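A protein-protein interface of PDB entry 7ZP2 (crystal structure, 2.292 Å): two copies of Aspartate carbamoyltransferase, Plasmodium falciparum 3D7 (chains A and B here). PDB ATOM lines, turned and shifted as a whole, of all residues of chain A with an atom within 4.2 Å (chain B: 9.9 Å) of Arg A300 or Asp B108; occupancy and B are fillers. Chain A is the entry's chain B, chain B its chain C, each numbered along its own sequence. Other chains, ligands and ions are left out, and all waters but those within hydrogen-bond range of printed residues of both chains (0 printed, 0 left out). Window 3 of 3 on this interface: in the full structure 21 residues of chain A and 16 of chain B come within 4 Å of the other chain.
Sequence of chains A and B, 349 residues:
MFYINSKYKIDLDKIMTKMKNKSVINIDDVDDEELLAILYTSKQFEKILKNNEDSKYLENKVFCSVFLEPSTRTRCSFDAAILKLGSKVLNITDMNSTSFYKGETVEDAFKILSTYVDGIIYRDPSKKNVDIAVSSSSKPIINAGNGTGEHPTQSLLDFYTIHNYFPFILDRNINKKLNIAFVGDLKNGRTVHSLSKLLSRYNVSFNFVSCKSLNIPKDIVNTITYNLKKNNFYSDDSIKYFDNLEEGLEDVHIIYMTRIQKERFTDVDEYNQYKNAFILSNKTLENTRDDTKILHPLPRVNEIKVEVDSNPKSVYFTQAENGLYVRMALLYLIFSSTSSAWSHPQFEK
Among the printed residues, merely in contact across the chains: Leu A298 with Ile B112, Pro A299 with Glu B104, Arg A300 with Gly B103, Val A301 with Gly B103, Phe A317 with Asp B108, Phe A317 with Lys B111 and Phe A317 with Ile B112.
The side-chain carboxylate of Asp B108 lies within salt-bridge range of the guanidinium group of Arg A300 (3.1 Å).
Of the 11 printed residues of chain A, 5 touch a printed residue of chain B. Along chain A the printed residues that touch a printed residue of chain B span positions 298 to 317. Of the 25 printed residues of chain B, 5 touch a printed residue of chain A. Among the printed residues, 8 pairs touch across the chains. Among the printed residues, Asp or Glu carboxylates within 4 Å of a Lys or Arg side-chain nitrogen of the other chain: Arg A300 with Asp B108 (3.1 Å).
The side-chain hydroxyl of Ser B114 sits at hydrogen-bond distance from the backbone carbonyl oxygen of Lys B111 (3.3 Å). The side-chain hydroxyl (OG1) of Thr B105 is in hydrogen-bond range of the backbone NH (N) of Asp B108 (3.0 Å). The guanidinium group of Arg A300 sits at hydrogen-bond distance from the backbone carbonyl oxygen of Ile A304, at 3.2 Å. The side-chain carboxylate (OD2) of Asp A309 lies within salt-bridge range of the guanidinium group (NH2) of Arg A300 (2.6 Å). OE2 of Glu A303 sits at hydrogen-bond distance from N of Val A301 (3.3 Å). The backbone carbonyl oxygen of Ile B112 lies within hydrogen-bond range of the side-chain hydroxyl of Thr B115 (2.5 Å).
Of the printed residues of chain B, Arg A300 touches Gly B103 and Asp B108. Of chain B, only Ile B112 (3.7 Å) comes within 4 Å of Leu A298. Pro A299 touches just one residue of chain B: Glu B104. No residue of chain B comes within 4 Å of Ile A304. No residue of chain B comes within 4 Å of Val A306. Of the printed residues of chain A, Ile B112 touches Leu A298 (3.7 Å) and Phe A317 (3.99 Å). Printed residues of chain A within 4 Å of Gly B103: Arg A300 (3.7 Å) and Val A301 (3.7 Å). Printed residues of chain B within 4 Å of Phe A317: Asp B108 (3.7 Å), Lys B111 (3.99 Å) and Ile B112 (3.99 Å). Of the printed residues of chain A, Glu B104 touches Pro A299 (3.5 Å). Of the printed residues of chain A, Lys B111 touches Phe A317. The nearest printed residue of chain A that does not touch Asp B108 is Asp A309 (4.9 Å).
No position is printed for both chains. Of the 8 pairs that touch across the chains among the printed residues, none has its exchanged pair printed and touching as well.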
ATOM      1  N   LEU A 298       5.238 -20.555 -10.021  1.00  0.00           N
ATOM      2  CA  LEU A 298       5.176 -19.362  -9.141  1.00  0.00           C
ATOM      3  C   LEU A 298       6.286 -19.474  -8.091  1.00  0.00           C
ATOM      4  O   LEU A 298       6.905 -20.524  -7.922  1.00  0.00           O
ATOM      5  CB  LEU A 298       3.780 -19.299  -8.517  1.00  0.00           C
ATOM      6  CG  LEU A 298       2.655 -19.171  -9.538  1.00  0.00           C
ATOM      7  CD1 LEU A 298       1.323 -19.223  -8.847  1.00  0.00           C
ATOM      8  CD2 LEU A 298       2.768 -17.885 -10.372  1.00  0.00           C
ATOM      9  N   PRO A 299       6.616 -18.389  -7.360  1.00  0.00           N
ATOM     10  CA  PRO A 299       6.067 -17.058  -7.599  1.00  0.00           C
ATOM     11  C   PRO A 299       6.544 -16.391  -8.897  1.00  0.00           C
ATOM     12  O   PRO A 299       7.536 -16.730  -9.522  1.00  0.00           O
ATOM     13  CB  PRO A 299       6.488 -16.241  -6.352  1.00  0.00           C
ATOM     14  CG  PRO A 299       7.707 -16.928  -5.898  1.00  0.00           C
ATOM     15  CD  PRO A 299       7.478 -18.398  -6.178  1.00  0.00           C
ATOM     16  N   ARG A 300       5.661 -15.492  -9.337  1.00  0.00           N
ATOM     17  CA  ARG A 300       5.744 -14.667 -10.548  1.00  0.00           C
ATOM     18  C   ARG A 300       6.431 -13.358 -10.139  1.00  0.00           C
ATOM     19  O   ARG A 300       6.155 -12.868  -8.991  1.00  0.00           O
ATOM     20  CB  ARG A 300       4.277 -14.558 -10.986  1.00  0.00           C
ATOM     21  CG  ARG A 300       4.013 -14.188 -12.431  1.00  0.00           C
ATOM     22  CD  ARG A 300       3.483 -12.758 -12.634  1.00  0.00           C
ATOM     23  NE  ARG A 300       2.191 -12.352 -12.092  1.00  0.00           N
ATOM     24  CZ  ARG A 300       1.136 -12.003 -12.837  1.00  0.00           C
ATOM     25  NH1 ARG A 300       1.153 -12.135 -14.159  1.00  0.00           N
ATOM     26  NH2 ARG A 300       0.022 -11.626 -12.247  1.00  0.00           N
ATOM     27  N   VAL A 301       7.314 -12.849 -10.988  1.00  0.00           N
ATOM     28  CA  VAL A 301       7.964 -11.521 -10.820  1.00  0.00           C
ATOM     29  C   VAL A 301       7.569 -10.714 -12.052  1.00  0.00           C
ATOM     30  O   VAL A 301       6.523 -10.034 -12.006  1.00  0.00           O
ATOM     31  CB  VAL A 301       9.493 -11.657 -10.609  1.00  0.00           C
ATOM     32  CG1 VAL A 301      10.261 -10.371 -10.831  1.00  0.00           C
ATOM     33  CG2 VAL A 301       9.800 -12.182  -9.212  1.00  0.00           C
ATOM     34  N   GLU A 303       8.341 -12.288 -15.341  1.00  0.00           N
ATOM     35  CA  GLU A 303       8.365 -13.330 -16.402  1.00  0.00           C
ATOM     36  C   GLU A 303       7.108 -13.248 -17.264  1.00  0.00           C
ATOM     37  O   GLU A 303       7.116 -13.688 -18.402  1.00  0.00           O
ATOM     38  CB  GLU A 303       8.415 -14.742 -15.835  1.00  0.00           C
ATOM     39  CG  GLU A 303       9.663 -14.994 -15.009  1.00  0.00           C
ATOM     40  CD  GLU A 303       9.434 -14.891 -13.504  1.00  0.00           C
ATOM     41  OE1 GLU A 303      10.341 -14.513 -12.786  1.00  0.00           O
ATOM     42  OE2 GLU A 303       8.373 -15.264 -13.032  1.00  0.00           O
ATOM     43  N   ILE A 304       6.003 -12.863 -16.644  1.00  0.00           N
ATOM     44  CA  ILE A 304       4.646 -12.723 -17.254  1.00  0.00           C
ATOM     45  C   ILE A 304       4.045 -11.385 -16.835  1.00  0.00           C
ATOM     46  O   ILE A 304       3.871 -11.162 -15.615  1.00  0.00           O
ATOM     47  CB  ILE A 304       3.744 -13.886 -16.806  1.00  0.00           C
ATOM     48  CG1 ILE A 304       4.377 -15.248 -17.106  1.00  0.00           C
ATOM     49  CG2 ILE A 304       2.379 -13.764 -17.436  1.00  0.00           C
ATOM     50  CD1 ILE A 304       3.474 -16.417 -16.877  1.00  0.00           C
ATOM     51  N   LYS A 305       3.671 -10.564 -17.810  1.00  0.00           N
ATOM     52  CA  LYS A 305       3.053  -9.224 -17.568  1.00  0.00           C
ATOM     53  C   LYS A 305       1.608  -9.419 -17.095  1.00  0.00           C
ATOM     54  O   LYS A 305       0.914 -10.331 -17.614  1.00  0.00           O
ATOM     55  CB  LYS A 305       3.107  -8.362 -18.834  1.00  0.00           C
ATOM     56  CG  LYS A 305       4.519  -7.933 -19.241  1.00  0.00           C
ATOM     57  CD  LYS A 305       4.648  -7.276 -20.586  1.00  0.00           C
ATOM     58  CE  LYS A 305       6.030  -7.426 -21.196  1.00  0.00           C
ATOM     59  NZ  LYS A 305       6.224  -6.577 -22.408  1.00  0.00           N
ATOM     60  N   VAL A 306       1.177  -8.559 -16.176  1.00  0.00           N
ATOM     61  CA  VAL A 306      -0.158  -8.625 -15.533  1.00  0.00           C
ATOM     62  C   VAL A 306      -1.255  -8.670 -16.609  1.00  0.00           C
ATOM     63  O   VAL A 306      -2.301  -9.266 -16.319  1.00  0.00           O
ATOM     64  CB  VAL A 306      -0.330  -7.480 -14.518  1.00  0.00           C
ATOM     65  CG1 VAL A 306      -1.791  -7.261 -14.116  1.00  0.00           C
ATOM     66  CG2 VAL A 306       0.534  -7.735 -13.271  1.00  0.00           C
ATOM     67  N   ASP A 309      -2.944 -12.059 -17.414  1.00  0.00           N
ATOM     68  CA  ASP A 309      -3.875 -12.649 -16.398  1.00  0.00           C
ATOM     69  C   ASP A 309      -5.317 -12.670 -16.945  1.00  0.00           C
ATOM     70  O   ASP A 309      -6.071 -13.573 -16.601  1.00  0.00           O
ATOM     71  CB  ASP A 309      -3.783 -11.901 -15.062  1.00  0.00           C
ATOM     72  CG  ASP A 309      -2.384 -11.861 -14.461  1.00  0.00           C
ATOM     73  OD1 ASP A 309      -1.487 -12.597 -14.986  1.00  0.00           O
ATOM     74  OD2 ASP A 309      -2.172 -11.118 -13.467  1.00  0.00           O
ATOM     75  N   TYR A 316      -2.034 -20.242 -14.679  1.00  0.00           N
ATOM     76  CA  TYR A 316      -1.005 -20.453 -13.612  1.00  0.00           C
ATOM     77  C   TYR A 316      -1.606 -20.302 -12.201  1.00  0.00           C
ATOM     78  O   TYR A 316      -1.080 -20.966 -11.246  1.00  0.00           O
ATOM     79  CB  TYR A 316       0.216 -19.530 -13.778  1.00  0.00           C
ATOM     80  CG  TYR A 316      -0.084 -18.218 -14.438  1.00  0.00           C
ATOM     81  CD1 TYR A 316      -0.532 -17.107 -13.726  1.00  0.00           C
ATOM     82  CD2 TYR A 316       0.044 -18.094 -15.809  1.00  0.00           C
ATOM     83  CE1 TYR A 316      -0.795 -15.893 -14.390  1.00  0.00           C
ATOM     84  CE2 TYR A 316      -0.246 -16.907 -16.466  1.00  0.00           C
ATOM     85  CZ  TYR A 316      -0.678 -15.804 -15.766  1.00  0.00           C
ATOM     86  OH  TYR A 316      -0.968 -14.640 -16.476  1.00  0.00           O
ATOM     87  N   PHE A 317      -2.691 -19.563 -12.043  1.00  0.00           N
ATOM     88  CA  PHE A 317      -3.451 -19.419 -10.780  1.00  0.00           C
ATOM     89  C   PHE A 317      -4.345 -20.640 -10.578  1.00  0.00           C
ATOM     90  O   PHE A 317      -4.341 -21.135  -9.443  1.00  0.00           O
ATOM     91  CB  PHE A 317      -4.326 -18.176 -10.749  1.00  0.00           C
ATOM     92  CG  PHE A 317      -3.557 -16.891 -10.803  1.00  0.00           C
ATOM     93  CD1 PHE A 317      -2.695 -16.560  -9.779  1.00  0.00           C
ATOM     94  CD2 PHE A 317      -3.756 -15.995 -11.831  1.00  0.00           C
ATOM     95  CE1 PHE A 317      -2.020 -15.351  -9.797  1.00  0.00           C
ATOM     96  CE2 PHE A 317      -3.111 -14.763 -11.826  1.00  0.00           C
ATOM     97  CZ  PHE A 317      -2.239 -14.442 -10.806  1.00  0.00           C
ATOM     98  N   PHE B 100       7.343 -11.922   3.696  1.00  0.00           N
ATOM     99  CA  PHE B 100       6.183 -12.712   3.218  1.00  0.00           C
ATOM    100  C   PHE B 100       5.933 -12.431   1.728  1.00  0.00           C
ATOM    101  O   PHE B 100       5.504 -13.346   1.039  1.00  0.00           O
ATOM    102  CB  PHE B 100       4.958 -12.417   4.077  1.00  0.00           C
ATOM    103  CG  PHE B 100       3.665 -13.025   3.596  1.00  0.00           C
ATOM    104  CD1 PHE B 100       3.390 -14.365   3.773  1.00  0.00           C
ATOM    105  CD2 PHE B 100       2.691 -12.229   3.024  1.00  0.00           C
ATOM    106  CE1 PHE B 100       2.160 -14.902   3.405  1.00  0.00           C
ATOM    107  CE2 PHE B 100       1.470 -12.763   2.631  1.00  0.00           C
ATOM    108  CZ  PHE B 100       1.199 -14.099   2.833  1.00  0.00           C
ATOM    109  N   TYR B 101       6.184 -11.206   1.255  1.00  0.00           N
ATOM    110  CA  TYR B 101       5.929 -10.757  -0.147  1.00  0.00           C
ATOM    111  C   TYR B 101       7.250 -10.778  -0.934  1.00  0.00           C
ATOM    112  O   TYR B 101       7.350 -10.132  -1.994  1.00  0.00           O
ATOM    113  CB  TYR B 101       5.242  -9.378  -0.148  1.00  0.00           C
ATOM    114  CG  TYR B 101       3.857  -9.373   0.473  1.00  0.00           C
ATOM    115  CD1 TYR B 101       2.863 -10.208  -0.013  1.00  0.00           C
ATOM    116  CD2 TYR B 101       3.537  -8.579   1.558  1.00  0.00           C
ATOM    117  CE1 TYR B 101       1.595 -10.223   0.533  1.00  0.00           C
ATOM    118  CE2 TYR B 101       2.279  -8.598   2.130  1.00  0.00           C
ATOM    119  CZ  TYR B 101       1.299  -9.430   1.616  1.00  0.00           C
ATOM    120  OH  TYR B 101       0.028  -9.503   2.129  1.00  0.00           O
ATOM    121  N   LYS B 102       8.241 -11.526  -0.433  1.00  0.00           N
ATOM    122  CA  LYS B 102       9.492 -11.947  -1.123  1.00  0.00           C
ATOM    123  C   LYS B 102       9.320 -11.814  -2.630  1.00  0.00           C
ATOM    124  O   LYS B 102       9.062 -12.859  -3.259  1.00  0.00           O
ATOM    125  CB  LYS B 102       9.832 -13.433  -0.863  1.00  0.00           C
ATOM    126  CG  LYS B 102      10.251 -13.792   0.559  1.00  0.00           C
ATOM    127  CD  LYS B 102      10.833 -15.205   0.702  1.00  0.00           C
ATOM    128  CE  LYS B 102       9.764 -16.278   0.702  1.00  0.00           C
ATOM    129  NZ  LYS B 102       8.904 -16.212   1.907  1.00  0.00           N
ATOM    130  N   GLY B 103       9.475 -10.617  -3.198  1.00  0.00           N
ATOM    131  CA  GLY B 103       9.336 -10.449  -4.655  1.00  0.00           C
ATOM    132  C   GLY B 103       8.089 -11.203  -5.123  1.00  0.00           C
ATOM    133  O   GLY B 103       8.153 -12.148  -5.910  1.00  0.00           O
ATOM    134  N   GLU B 104       6.969 -10.870  -4.522  1.00  0.00           N
ATOM    135  CA  GLU B 104       5.635 -11.253  -5.030  1.00  0.00           C
ATOM    136  C   GLU B 104       4.683 -10.131  -4.668  1.00  0.00           C
ATOM    137  O   GLU B 104       4.777  -9.625  -3.579  1.00  0.00           O
ATOM    138  CB  GLU B 104       5.147 -12.596  -4.493  1.00  0.00           C
ATOM    139  CG  GLU B 104       3.944 -13.088  -5.259  1.00  0.00           C
ATOM    140  CD  GLU B 104       3.444 -14.456  -4.824  1.00  0.00           C
ATOM    141  OE1 GLU B 104       3.363 -14.680  -3.595  1.00  0.00           O
ATOM    142  OE2 GLU B 104       3.139 -15.296  -5.723  1.00  0.00           O
ATOM    143  N   THR B 105       3.769  -9.810  -5.579  1.00  0.00           N
ATOM    144  CA  THR B 105       2.715  -8.794  -5.364  1.00  0.00           C
ATOM    145  C   THR B 105       1.733  -9.317  -4.310  1.00  0.00           C
ATOM    146  O   THR B 105       1.502 -10.533  -4.178  1.00  0.00           O
ATOM    147  CB  THR B 105       1.999  -8.456  -6.672  1.00  0.00           C
ATOM    148  OG1 THR B 105       1.314  -9.653  -7.042  1.00  0.00           O
ATOM    149  CG2 THR B 105       2.929  -7.966  -7.771  1.00  0.00           C
ATOM    150  N   VAL B 106       1.142  -8.391  -3.588  1.00  0.00           N
ATOM    151  CA  VAL B 106       0.082  -8.654  -2.601  1.00  0.00           C
ATOM    152  C   VAL B 106      -1.088  -9.297  -3.327  1.00  0.00           C
ATOM    153  O   VAL B 106      -1.666 -10.216  -2.762  1.00  0.00           O
ATOM    154  CB  VAL B 106      -0.268  -7.362  -1.851  1.00  0.00           C
ATOM    155  CG1 VAL B 106      -1.394  -7.554  -0.856  1.00  0.00           C
ATOM    156  CG2 VAL B 106       0.988  -6.834  -1.176  1.00  0.00           C
ATOM    157  N   GLU B 107      -1.350  -8.892  -4.568  1.00  0.00           N
ATOM    158  CA  GLU B 107      -2.515  -9.386  -5.335  1.00  0.00           C
ATOM    159  C   GLU B 107      -2.299 -10.860  -5.732  1.00  0.00           C
ATOM    160  O   GLU B 107      -3.288 -11.619  -5.719  1.00  0.00           O
ATOM    161  CB  GLU B 107      -2.936  -8.446  -6.473  1.00  0.00           C
ATOM    162  CG  GLU B 107      -1.885  -7.564  -7.099  1.00  0.00           C
ATOM    163  CD  GLU B 107      -1.587  -6.201  -6.478  1.00  0.00           C
ATOM    164  OE1 GLU B 107      -2.352  -5.221  -6.717  1.00  0.00           O
ATOM    165  OE2 GLU B 107      -0.545  -6.132  -5.793  1.00  0.00           O
ATOM    166  N   ASP B 108      -1.074 -11.250  -6.105  1.00  0.00           N
ATOM    167  CA  ASP B 108      -0.744 -12.649  -6.449  1.00  0.00           C
ATOM    168  C   ASP B 108      -0.943 -13.460  -5.188  1.00  0.00           C
ATOM    169  O   ASP B 108      -1.681 -14.441  -5.230  1.00  0.00           O
ATOM    170  CB  ASP B 108       0.673 -12.788  -7.008  1.00  0.00           C
ATOM    171  CG  ASP B 108       0.788 -12.449  -8.453  1.00  0.00           C
ATOM    172  OD1 ASP B 108      -0.222 -11.938  -8.995  1.00  0.00           O
ATOM    173  OD2 ASP B 108       1.815 -12.890  -9.014  1.00  0.00           O
ATOM    174  N   ALA B 109      -0.361 -13.005  -4.066  1.00  0.00           N
ATOM    175  CA  ALA B 109      -0.365 -13.787  -2.814  1.00  0.00           C
ATOM    176  C   ALA B 109      -1.815 -14.063  -2.393  1.00  0.00           C
ATOM    177  O   ALA B 109      -2.115 -15.168  -1.957  1.00  0.00           O
ATOM    178  CB  ALA B 109       0.400 -13.040  -1.769  1.00  0.00           C
ATOM    179  N   PHE B 110      -2.681 -13.057  -2.449  1.00  0.00           N
ATOM    180  CA  PHE B 110      -4.065 -13.194  -1.960  1.00  0.00           C
ATOM    181  C   PHE B 110      -4.953 -13.948  -2.959  1.00  0.00           C
ATOM    182  O   PHE B 110      -5.885 -14.689  -2.525  1.00  0.00           O
ATOM    183  CB  PHE B 110      -4.633 -11.839  -1.553  1.00  0.00           C
ATOM    184  CG  PHE B 110      -4.321 -11.604  -0.108  1.00  0.00           C
ATOM    185  CD1 PHE B 110      -3.104 -11.047   0.262  1.00  0.00           C
ATOM    186  CD2 PHE B 110      -5.147 -12.122   0.868  1.00  0.00           C
ATOM    187  CE1 PHE B 110      -2.763 -10.989   1.589  1.00  0.00           C
ATOM    188  CE2 PHE B 110      -4.828 -11.993   2.195  1.00  0.00           C
ATOM    189  CZ  PHE B 110      -3.629 -11.452   2.551  1.00  0.00           C
ATOM    190  N   LYS B 111      -4.679 -13.820  -4.237  1.00  0.00           N
ATOM    191  CA  LYS B 111      -5.475 -14.554  -5.246  1.00  0.00           C
ATOM    192  C   LYS B 111      -5.271 -16.063  -5.021  1.00  0.00           C
ATOM    193  O   LYS B 111      -6.251 -16.844  -5.144  1.00  0.00           O
ATOM    194  CB  LYS B 111      -5.119 -14.066  -6.655  1.00  0.00           C
ATOM    195  CG  LYS B 111      -5.954 -14.654  -7.776  1.00  0.00           C
ATOM    196  CD  LYS B 111      -6.294 -13.742  -8.923  1.00  0.00           C
ATOM    197  CE  LYS B 111      -6.992 -14.482 -10.045  1.00  0.00           C
ATOM    198  NZ  LYS B 111      -8.355 -14.978  -9.706  1.00  0.00           N
ATOM    199  N   ILE B 112      -4.062 -16.448  -4.695  1.00  0.00           N
ATOM    200  CA  ILE B 112      -3.671 -17.879  -4.526  1.00  0.00           C
ATOM    201  C   ILE B 112      -4.164 -18.364  -3.160  1.00  0.00           C
ATOM    202  O   ILE B 112      -4.877 -19.377  -3.095  1.00  0.00           O
ATOM    203  CB  ILE B 112      -2.147 -18.027  -4.668  1.00  0.00           C
ATOM    204  CG1 ILE B 112      -1.750 -17.864  -6.127  1.00  0.00           C
ATOM    205  CG2 ILE B 112      -1.632 -19.343  -4.108  1.00  0.00           C
ATOM    206  CD1 ILE B 112      -0.422 -17.196  -6.332  1.00  0.00           C
ATOM    207  N   LEU B 113      -3.847 -17.611  -2.109  1.00  0.00           N
ATOM    208  CA  LEU B 113      -4.153 -18.088  -0.761  1.00  0.00           C
ATOM    209  C   LEU B 113      -5.667 -18.330  -0.615  1.00  0.00           C
ATOM    210  O   LEU B 113      -6.058 -19.311   0.099  1.00  0.00           O
ATOM    211  CB  LEU B 113      -3.621 -17.037   0.198  1.00  0.00           C
ATOM    212  CG  LEU B 113      -3.828 -17.333   1.665  1.00  0.00           C
ATOM    213  CD1 LEU B 113      -3.095 -18.674   2.013  1.00  0.00           C
ATOM    214  CD2 LEU B 113      -3.325 -16.133   2.443  1.00  0.00           C
ATOM    215  N   SER B 114      -6.485 -17.518  -1.266  1.00  0.00           N
ATOM    216  CA  SER B 114      -7.951 -17.555  -1.083  1.00  0.00           C
ATOM    217  C   SER B 114      -8.523 -18.787  -1.792  1.00  0.00           C
ATOM    218  O   SER B 114      -9.660 -19.148  -1.478  1.00  0.00           O
ATOM    219  CB  SER B 114      -8.627 -16.266  -1.482  1.00  0.00           C
ATOM    220  OG  SER B 114      -8.265 -15.869  -2.773  1.00  0.00           O
ATOM    221  N   THR B 115      -7.739 -19.445  -2.665  1.00  0.00           N
ATOM    222  CA  THR B 115      -8.184 -20.703  -3.316  1.00  0.00           C
ATOM    223  C   THR B 115      -8.097 -21.819  -2.263  1.00  0.00           C
ATOM    224  O   THR B 115      -8.843 -22.781  -2.409  1.00  0.00           O
ATOM    225  CB  THR B 115      -7.443 -20.914  -4.633  1.00  0.00           C
ATOM    226  OG1 THR B 115      -6.026 -21.105  -4.483  1.00  0.00           O
ATOM    227  CG2 THR B 115      -7.688 -19.751  -5.579  1.00  0.00           C
ATOM    228  N   TYR B 116      -7.332 -21.667  -1.182  1.00  0.00           N
ATOM    229  CA  TYR B 116      -7.051 -22.775  -0.256  1.00  0.00           C
ATOM    230  C   TYR B 116      -8.103 -22.869   0.830  1.00  0.00           C
ATOM    231  O   TYR B 116      -8.081 -23.905   1.466  1.00  0.00           O
ATOM    232  CB  TYR B 116      -5.694 -22.640   0.458  1.00  0.00           C
ATOM    233  CG  TYR B 116      -4.471 -22.692  -0.435  1.00  0.00           C
ATOM    234  CD1 TYR B 116      -4.560 -23.219  -1.698  1.00  0.00           C
ATOM    235  CD2 TYR B 116      -3.248 -22.208  -0.013  1.00  0.00           C
ATOM    236  CE1 TYR B 116      -3.451 -23.319  -2.521  1.00  0.00           C
ATOM    237  CE2 TYR B 116      -2.138 -22.223  -0.845  1.00  0.00           C
ATOM    238  CZ  TYR B 116      -2.251 -22.748  -2.131  1.00  0.00           C
ATOM    239  OH  TYR B 116      -1.201 -22.777  -3.028  1.00  0.00           O
ATOM    240  N   ILE B 120     -10.098 -15.394   5.461  1.00  0.00           N
ATOM    241  CA  ILE B 120      -8.741 -14.931   5.807  1.00  0.00           C
ATOM    242  C   ILE B 120      -8.919 -13.864   6.862  1.00  0.00           C
ATOM    243  O   ILE B 120      -9.708 -13.005   6.646  1.00  0.00           O
ATOM    244  CB  ILE B 120      -7.996 -14.383   4.573  1.00  0.00           C
ATOM    245  CG1 ILE B 120      -7.814 -15.430   3.465  1.00  0.00           C
ATOM    246  CG2 ILE B 120      -6.700 -13.715   4.959  1.00  0.00           C
ATOM    247  CD1 ILE B 120      -7.755 -14.757   2.094  1.00  0.00           C
ATOM    248  N   ASN B 129      -1.880  -2.688   1.889  1.00  0.00           N
ATOM    249  CA  ASN B 129      -1.869  -4.172   1.781  1.00  0.00           C
ATOM    250  C   ASN B 129      -3.284  -4.734   2.013  1.00  0.00           C
ATOM    251  O   ASN B 129      -3.711  -5.580   1.235  1.00  0.00           O
ATOM    252  CB  ASN B 129      -0.802  -4.773   2.677  1.00  0.00           C
ATOM    253  CG  ASN B 129       0.602  -4.535   2.144  1.00  0.00           C
ATOM    254  OD1 ASN B 129       1.628  -4.827   2.791  1.00  0.00           O
ATOM    255  ND2 ASN B 129       0.657  -3.983   0.962  1.00  0.00           N
ATOM    256  N   ILE B 132      -5.592  -3.983  -0.911  1.00  0.00           N
ATOM    257  CA  ILE B 132      -5.191  -4.811  -2.085  1.00  0.00           C
ATOM    258  C   ILE B 132      -5.633  -6.262  -1.852  1.00  0.00           C
ATOM    259  O   ILE B 132      -6.145  -6.871  -2.799  1.00  0.00           O
ATOM    260  CB  ILE B 132      -3.683  -4.664  -2.373  1.00  0.00           C
ATOM    261  CG1 ILE B 132      -3.360  -3.278  -2.942  1.00  0.00           C
ATOM    262  CG2 ILE B 132      -3.225  -5.720  -3.336  1.00  0.00           C
ATOM    263  CD1 ILE B 132      -1.884  -2.941  -2.938  1.00  0.00           C
ATOM    264  N   ALA B 133      -5.452  -6.797  -0.648  1.00  0.00           N
ATOM    265  CA  ALA B 133      -5.891  -8.166  -0.286  1.00  0.00           C
ATOM    266  C   ALA B 133      -7.369  -8.328  -0.613  1.00  0.00           C
ATOM    267  O   ALA B 133      -7.750  -9.314  -1.252  1.00  0.00           O
ATOM    268  CB  ALA B 133      -5.613  -8.451   1.175  1.00  0.00           C
ATOM    269  N   SER B 135      -9.359  -6.615  -2.671  1.00  0.00           N
ATOM    270  CA  SER B 135      -9.522  -6.543  -4.149  1.00  0.00           C
ATOM    271  C   SER B 135      -9.138  -7.864  -4.817  1.00  0.00           C
ATOM    272  O   SER B 135      -9.703  -8.155  -5.873  1.00  0.00           O
ATOM    273  CB  SER B 135      -8.701  -5.429  -4.776  1.00  0.00           C
ATOM    274  OG  SER B 135      -8.474  -4.356  -3.884  1.00  0.00           O
ATOM    275  N   SER B 136      -8.135  -8.563  -4.290  1.00  0.00           N
ATOM    276  CA  SER B 136      -7.525  -9.720  -4.995  1.00  0.00           C
ATOM    277  C   SER B 136      -8.164 -11.031  -4.565  1.00  0.00           C
ATOM    278  O   SER B 136      -7.978 -11.979  -5.324  1.00  0.00           O
ATOM    279  CB  SER B 136      -6.050  -9.779  -4.761  1.00  0.00           C
ATOM    280  OG  SER B 136      -5.462  -8.578  -5.192  1.00  0.00           O
ATOM    281  N   SER B 137      -8.770 -11.068  -3.360  1.00  0.00           N
ATOM    282  CA  SER B 137      -9.213 -12.306  -2.690  1.00  0.00           C
ATOM    283  C   SER B 137     -10.527 -12.782  -3.305  1.00  0.00           C
ATOM    284  O   SER B 137     -11.447 -11.925  -3.389  1.00  0.00           O
ATOM    285  CB  SER B 137      -9.370 -12.078  -1.210  1.00  0.00           C
ATOM    286  OG  SER B 137      -9.847 -13.236  -0.544  1.00  0.00           O
ATOM    287  N   SER B 138     -10.670 -14.097  -3.546  1.00  0.00           N
ATOM    288  CA  SER B 138     -11.991 -14.677  -3.886  1.00  0.00           C
ATOM    289  C   SER B 138     -12.785 -14.944  -2.615  1.00  0.00           C
ATOM    290  O   SER B 138     -13.965 -15.351  -2.698  1.00  0.00           O
ATOM    291  CB  SER B 138     -11.839 -15.925  -4.748  1.00  0.00           C
ATOM    292  OG  SER B 138     -10.945 -16.830  -4.131  1.00  0.00           O
